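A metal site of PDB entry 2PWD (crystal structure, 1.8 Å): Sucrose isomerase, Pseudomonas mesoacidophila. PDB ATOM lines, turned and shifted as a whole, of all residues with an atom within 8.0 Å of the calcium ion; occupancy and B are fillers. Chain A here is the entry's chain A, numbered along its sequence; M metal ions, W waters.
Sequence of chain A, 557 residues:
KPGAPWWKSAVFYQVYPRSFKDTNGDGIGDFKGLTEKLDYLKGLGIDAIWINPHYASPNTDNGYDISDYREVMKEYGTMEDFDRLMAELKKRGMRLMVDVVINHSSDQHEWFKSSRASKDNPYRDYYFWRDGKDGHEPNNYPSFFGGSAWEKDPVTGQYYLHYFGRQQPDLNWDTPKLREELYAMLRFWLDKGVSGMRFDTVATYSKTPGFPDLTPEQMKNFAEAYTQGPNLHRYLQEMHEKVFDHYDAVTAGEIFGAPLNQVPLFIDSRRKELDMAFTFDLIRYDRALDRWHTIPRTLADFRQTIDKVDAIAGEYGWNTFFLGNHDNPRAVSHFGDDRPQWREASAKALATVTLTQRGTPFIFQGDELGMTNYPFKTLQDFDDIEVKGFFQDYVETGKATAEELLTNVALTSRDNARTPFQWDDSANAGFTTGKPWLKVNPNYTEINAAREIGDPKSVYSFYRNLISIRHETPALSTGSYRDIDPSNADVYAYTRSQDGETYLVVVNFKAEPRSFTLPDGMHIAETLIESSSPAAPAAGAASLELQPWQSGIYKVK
The nearest printed residue that does not touch the calcium ion is Thr 23 (4.2 Å).
Water W1 bridges O of Glu 75 (3.1 Å) and ND2 of Asn 24 (3.3 Å). Water W2 bridges O of Glu 75 (2.5 Å) and OD2 of Asp 26 (2.6 Å).
The calcium ion is bound by the side-chain amide oxygen (OD1) of Asn 24 (2.2 Å), the side-chain carboxylate (OD1) of Asp 22 (2.2 Å), the side-chain carboxylate (OD2) of Asp 30 (2.3 Å), the backbone carbonyl oxygen (O) of Ile 28 (2.3 Å), water W2 (2.4 Å), the side-chain carboxylate (OD1) of Asp 26 (2.4 Å) and water W1 (2.5 Å).
The side-chain carboxylate (OD2) of Asp 22 sits at hydrogen-bond distance from the backbone NH (N) of Gly 25, at 3.2 Å. N of Gly 27 is in hydrogen-bond range of OD2 of Asp 22 (2.8 Å). The side-chain hydroxyl (OG1) of Thr 432 is in hydrogen-bond range of the side-chain carboxylate (OD2) of Asp 22 (2.6 Å). N of Asp 22 lies within hydrogen-bond range of O of Phe 431. OG1 of Thr 23 is in hydrogen-bond range of OD1 of Asp 30 (2.6 Å). N of Asp 30 lies within hydrogen-bond range of O of Lys 21, at 3.0 Å. OD1 of Asp 30 sits at hydrogen-bond distance from N of Gly 33 (2.9 Å).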
ATOM      1  N   PRO A  17     -21.337  -0.663  25.710  1.00  0.00           N
ATOM      2  CA  PRO A  17     -21.656   0.076  24.484  1.00  0.00           C
ATOM      3  C   PRO A  17     -22.904  -0.324  23.713  1.00  0.00           C
ATOM      4  O   PRO A  17     -23.706   0.536  23.342  1.00  0.00           O
ATOM      5  CB  PRO A  17     -20.378  -0.060  23.635  1.00  0.00           C
ATOM      6  CG  PRO A  17     -19.299  -0.149  24.671  1.00  0.00           C
ATOM      7  CD  PRO A  17     -19.934  -1.135  25.673  1.00  0.00           C
ATOM      8  N   ARG A  18     -23.047  -1.615  23.484  1.00  0.00           N
ATOM      9  CA  ARG A  18     -24.180  -2.170  22.762  1.00  0.00           C
ATOM     10  C   ARG A  18     -25.514  -1.655  23.312  1.00  0.00           C
ATOM     11  O   ARG A  18     -26.488  -1.500  22.566  1.00  0.00           O
ATOM     12  CB  ARG A  18     -24.109  -3.686  22.893  1.00  0.00           C
ATOM     13  CG  ARG A  18     -25.066  -4.448  22.057  1.00  0.00           C
ATOM     14  CD  ARG A  18     -24.900  -5.935  22.326  1.00  0.00           C
ATOM     15  NE  ARG A  18     -25.795  -6.662  21.447  1.00  0.00           N
ATOM     16  CZ  ARG A  18     -25.501  -6.986  20.193  1.00  0.00           C
ATOM     17  NH1 ARG A  18     -24.335  -6.656  19.673  1.00  0.00           N
ATOM     18  NH2 ARG A  18     -26.407  -7.619  19.455  1.00  0.00           N
ATOM     19  N   LYS A  21     -26.026   3.913  24.060  1.00  0.00           N
ATOM     20  CA  LYS A  21     -26.687   4.928  23.214  1.00  0.00           C
ATOM     21  C   LYS A  21     -26.440   4.688  21.734  1.00  0.00           C
ATOM     22  O   LYS A  21     -25.288   4.676  21.262  1.00  0.00           O
ATOM     23  CB  LYS A  21     -26.199   6.322  23.590  1.00  0.00           C
ATOM     24  CG  LYS A  21     -26.709   7.435  22.683  1.00  0.00           C
ATOM     25  CD  LYS A  21     -28.205   7.650  22.823  1.00  0.00           C
ATOM     26  CE  LYS A  21     -28.664   8.786  21.922  1.00  0.00           C
ATOM     27  NZ  LYS A  21     -30.103   9.046  22.047  1.00  0.00           N
ATOM     28  N   ASP A  22     -27.528   4.484  20.989  1.00  0.00           N
ATOM     29  CA  ASP A  22     -27.466   4.230  19.551  1.00  0.00           C
ATOM     30  C   ASP A  22     -27.657   5.563  18.824  1.00  0.00           C
ATOM     31  O   ASP A  22     -28.508   6.361  19.209  1.00  0.00           O
ATOM     32  CB  ASP A  22     -28.589   3.254  19.159  1.00  0.00           C
ATOM     33  CG  ASP A  22     -28.683   3.010  17.660  1.00  0.00           C
ATOM     34  OD1 ASP A  22     -27.667   3.152  16.938  1.00  0.00           O
ATOM     35  OD2 ASP A  22     -29.787   2.655  17.191  1.00  0.00           O
ATOM     36  N   THR A  23     -26.873   5.812  17.782  1.00  0.00           N
ATOM     37  CA  THR A  23     -26.990   7.061  17.042  1.00  0.00           C
ATOM     38  C   THR A  23     -27.327   6.890  15.572  1.00  0.00           C
ATOM     39  O   THR A  23     -27.424   7.865  14.827  1.00  0.00           O
ATOM     40  CB  THR A  23     -25.705   7.904  17.147  1.00  0.00           C
ATOM     41  OG1 THR A  23     -24.575   7.105  16.766  1.00  0.00           O
ATOM     42  CG2 THR A  23     -25.534   8.433  18.562  1.00  0.00           C
ATOM     43  N   ASN A  24     -27.523   5.651  15.116  1.00  0.00           N
ATOM     44  CA  ASN A  24     -27.840   5.457  13.713  1.00  0.00           C
ATOM     45  C   ASN A  24     -29.063   4.574  13.479  1.00  0.00           C
ATOM     46  O   ASN A  24     -29.271   4.066  12.395  1.00  0.00           O
ATOM     47  CB  ASN A  24     -26.610   4.919  12.966  1.00  0.00           C
ATOM     48  CG  ASN A  24     -26.298   3.491  13.302  1.00  0.00           C
ATOM     49  OD1 ASN A  24     -26.509   3.059  14.431  1.00  0.00           O
ATOM     50  ND2 ASN A  24     -25.776   2.748  12.338  1.00  0.00           N
ATOM     51  N   GLY A  25     -29.874   4.400  14.525  1.00  0.00           N
ATOM     52  CA  GLY A  25     -31.092   3.625  14.391  1.00  0.00           C
ATOM     53  C   GLY A  25     -31.033   2.145  14.100  1.00  0.00           C
ATOM     54  O   GLY A  25     -32.052   1.547  13.762  1.00  0.00           O
ATOM     55  N   ASP A  26     -29.871   1.513  14.221  1.00  0.00           N
ATOM     56  CA  ASP A  26     -29.827   0.082  13.957  1.00  0.00           C
ATOM     57  C   ASP A  26     -30.167  -0.688  15.235  1.00  0.00           C
ATOM     58  O   ASP A  26     -30.176  -1.918  15.235  1.00  0.00           O
ATOM     59  CB  ASP A  26     -28.444  -0.329  13.384  1.00  0.00           C
ATOM     60  CG  ASP A  26     -27.314  -0.178  14.390  1.00  0.00           C
ATOM     61  OD1 ASP A  26     -27.500   0.486  15.422  1.00  0.00           O
ATOM     62  OD2 ASP A  26     -26.209  -0.723  14.113  1.00  0.00           O
ATOM     63  N   GLY A  27     -30.478   0.040  16.309  1.00  0.00           N
ATOM     64  CA  GLY A  27     -30.850  -0.594  17.569  1.00  0.00           C
ATOM     65  C   GLY A  27     -29.685  -1.058  18.430  1.00  0.00           C
ATOM     66  O   GLY A  27     -29.875  -1.726  19.455  1.00  0.00           O
ATOM     67  N   ILE A  28     -28.469  -0.712  18.008  1.00  0.00           N
ATOM     68  CA  ILE A  28     -27.281  -1.102  18.758  1.00  0.00           C
ATOM     69  C   ILE A  28     -26.484   0.143  19.148  1.00  0.00           C
ATOM     70  O   ILE A  28     -26.231   1.017  18.323  1.00  0.00           O
ATOM     71  CB  ILE A  28     -26.405  -2.061  17.942  1.00  0.00           C
ATOM     72  CG1 ILE A  28     -27.181  -3.339  17.632  1.00  0.00           C
ATOM     73  CG2 ILE A  28     -25.154  -2.393  18.721  1.00  0.00           C
ATOM     74  CD1 ILE A  28     -26.470  -4.282  16.683  1.00  0.00           C
ATOM     75  N   GLY A  29     -26.102   0.226  20.424  1.00  0.00           N
ATOM     76  CA  GLY A  29     -25.336   1.351  20.903  1.00  0.00           C
ATOM     77  C   GLY A  29     -24.024   1.434  20.173  1.00  0.00           C
ATOM     78  O   GLY A  29     -23.535   0.448  19.646  1.00  0.00           O
ATOM     79  N   ASP A  30     -23.413   2.609  20.157  1.00  0.00           N
ATOM     80  CA  ASP A  30     -22.175   2.755  19.418  1.00  0.00           C
ATOM     81  C   ASP A  30     -21.264   3.798  20.035  1.00  0.00           C
ATOM     82  O   ASP A  30     -21.611   4.421  21.019  1.00  0.00           O
ATOM     83  CB  ASP A  30     -22.519   3.099  17.954  1.00  0.00           C
ATOM     84  CG  ASP A  30     -23.661   4.107  17.849  1.00  0.00           C
ATOM     85  OD1 ASP A  30     -23.504   5.255  18.329  1.00  0.00           O
ATOM     86  OD2 ASP A  30     -24.725   3.760  17.271  1.00  0.00           O
ATOM     87  N   PHE A  31     -20.078   3.956  19.460  1.00  0.00           N
ATOM     88  CA  PHE A  31     -19.115   4.926  19.977  1.00  0.00           C
ATOM     89  C   PHE A  31     -19.619   6.355  19.903  1.00  0.00           C
ATOM     90  O   PHE A  31     -19.427   7.133  20.836  1.00  0.00           O
ATOM     91  CB  PHE A  31     -17.803   4.843  19.232  1.00  0.00           C
ATOM     92  CG  PHE A  31     -16.998   3.621  19.539  1.00  0.00           C
ATOM     93  CD1 PHE A  31     -16.803   3.215  20.851  1.00  0.00           C
ATOM     94  CD2 PHE A  31     -16.399   2.896  18.513  1.00  0.00           C
ATOM     95  CE1 PHE A  31     -15.995   2.107  21.144  1.00  0.00           C
ATOM     96  CE2 PHE A  31     -15.598   1.786  18.799  1.00  0.00           C
ATOM     97  CZ  PHE A  31     -15.402   1.400  20.117  1.00  0.00           C
ATOM     98  N   LYS A  32     -20.234   6.734  18.792  1.00  0.00           N
ATOM     99  CA  LYS A  32     -20.743   8.099  18.711  1.00  0.00           C
ATOM    100  C   LYS A  32     -21.749   8.343  19.826  1.00  0.00           C
ATOM    101  O   LYS A  32     -21.788   9.413  20.397  1.00  0.00           O
ATOM    102  CB  LYS A  32     -21.401   8.357  17.353  1.00  0.00           C
ATOM    103  CG  LYS A  32     -20.416   8.582  16.214  1.00  0.00           C
ATOM    104  CD  LYS A  32     -21.141   9.052  14.963  1.00  0.00           C
ATOM    105  CE  LYS A  32     -20.162   9.358  13.823  1.00  0.00           C
ATOM    106  NZ  LYS A  32     -19.444   8.143  13.352  1.00  0.00           N
ATOM    107  N   GLY A  33     -22.556   7.334  20.146  1.00  0.00           N
ATOM    108  CA  GLY A  33     -23.531   7.502  21.215  1.00  0.00           C
ATOM    109  C   GLY A  33     -22.832   7.728  22.548  1.00  0.00           C
ATOM    110  O   GLY A  33     -23.213   8.614  23.308  1.00  0.00           O
ATOM    111  N   LYS A  74     -17.472  -3.318  14.030  1.00  0.00           N
ATOM    112  CA  LYS A  74     -18.225  -2.610  13.003  1.00  0.00           C
ATOM    113  C   LYS A  74     -19.455  -1.903  13.571  1.00  0.00           C
ATOM    114  O   LYS A  74     -19.704  -0.737  13.271  1.00  0.00           O
ATOM    115  CB  LYS A  74     -18.637  -3.594  11.888  1.00  0.00           C
ATOM    116  N   GLU A  75     -20.214  -2.595  14.424  1.00  0.00           N
ATOM    117  CA  GLU A  75     -21.409  -2.022  15.047  1.00  0.00           C
ATOM    118  C   GLU A  75     -21.130  -0.751  15.854  1.00  0.00           C
ATOM    119  O   GLU A  75     -21.969   0.153  15.898  1.00  0.00           O
ATOM    120  CB  GLU A  75     -22.078  -3.019  15.988  1.00  0.00           C
ATOM    121  CG  GLU A  75     -22.826  -4.166  15.333  1.00  0.00           C
ATOM    122  CD  GLU A  75     -21.916  -5.124  14.606  1.00  0.00           C
ATOM    123  OE1 GLU A  75     -20.803  -5.396  15.105  1.00  0.00           O
ATOM    124  OE2 GLU A  75     -22.325  -5.631  13.548  1.00  0.00           O
ATOM    125  N   TYR A  76     -19.979  -0.668  16.514  1.00  0.00           N
ATOM    126  CA  TYR A  76     -19.692   0.512  17.322  1.00  0.00           C
ATOM    127  C   TYR A  76     -19.124   1.706  16.568  1.00  0.00           C
ATOM    128  O   TYR A  76     -19.167   2.825  17.068  1.00  0.00           O
ATOM    129  CB  TYR A  76     -18.757   0.175  18.498  1.00  0.00           C
ATOM    130  CG  TYR A  76     -19.300  -0.862  19.454  1.00  0.00           C
ATOM    131  CD1 TYR A  76     -20.639  -1.254  19.392  1.00  0.00           C
ATOM    132  CD2 TYR A  76     -18.471  -1.481  20.390  1.00  0.00           C
ATOM    133  CE1 TYR A  76     -21.136  -2.251  20.239  1.00  0.00           C
ATOM    134  CE2 TYR A  76     -18.960  -2.456  21.253  1.00  0.00           C
ATOM    135  CZ  TYR A  76     -20.291  -2.846  21.170  1.00  0.00           C
ATOM    136  OH  TYR A  76     -20.791  -3.803  22.024  1.00  0.00           O
ATOM    137  N   GLY A  77     -18.603   1.472  15.376  1.00  0.00           N
ATOM    138  CA  GLY A  77     -18.051   2.568  14.592  1.00  0.00           C
ATOM    139  C   GLY A  77     -16.757   2.204  13.923  1.00  0.00           C
ATOM    140  O   GLY A  77     -16.546   1.049  13.571  1.00  0.00           O
ATOM    141  N   PHE A 431     -33.037   5.589  23.689  1.00  0.00           N
ATOM    142  CA  PHE A 431     -31.826   4.813  23.381  1.00  0.00           C
ATOM    143  C   PHE A 431     -31.614   4.728  21.868  1.00  0.00           C
ATOM    144  O   PHE A 431     -30.485   4.843  21.373  1.00  0.00           O
ATOM    145  CB  PHE A 431     -31.960   3.392  23.943  1.00  0.00           C
ATOM    146  CG  PHE A 431     -30.968   2.418  23.361  1.00  0.00           C
ATOM    147  CD1 PHE A 431     -29.612   2.512  23.682  1.00  0.00           C
ATOM    148  CD2 PHE A 431     -31.385   1.430  22.481  1.00  0.00           C
ATOM    149  CE1 PHE A 431     -28.704   1.621  23.133  1.00  0.00           C
ATOM    150  CE2 PHE A 431     -30.480   0.528  21.924  1.00  0.00           C
ATOM    151  CZ  PHE A 431     -29.134   0.629  22.251  1.00  0.00           C
ATOM    152  N   THR A 432     -32.709   4.543  21.137  1.00  0.00           N
ATOM    153  CA  THR A 432     -32.613   4.390  19.689  1.00  0.00           C
ATOM    154  C   THR A 432     -33.871   4.918  18.987  1.00  0.00           C
ATOM    155  O   THR A 432     -34.919   5.054  19.621  1.00  0.00           O
ATOM    156  CB  THR A 432     -32.425   2.900  19.327  1.00  0.00           C
ATOM    157  OG1 THR A 432     -32.237   2.740  17.925  1.00  0.00           O
ATOM    158  CG2 THR A 432     -33.627   2.083  19.779  1.00  0.00           C
HETATM  159 CA    CA M   1     -25.854   2.073  16.287  1.00  0.00          CA
HETATM  160  O   HOH W   1     -23.824   2.473  14.935  1.00  0.00           O
HETATM  161  O   HOH W   2     -24.453   0.185  15.839  1.00  0.00           O
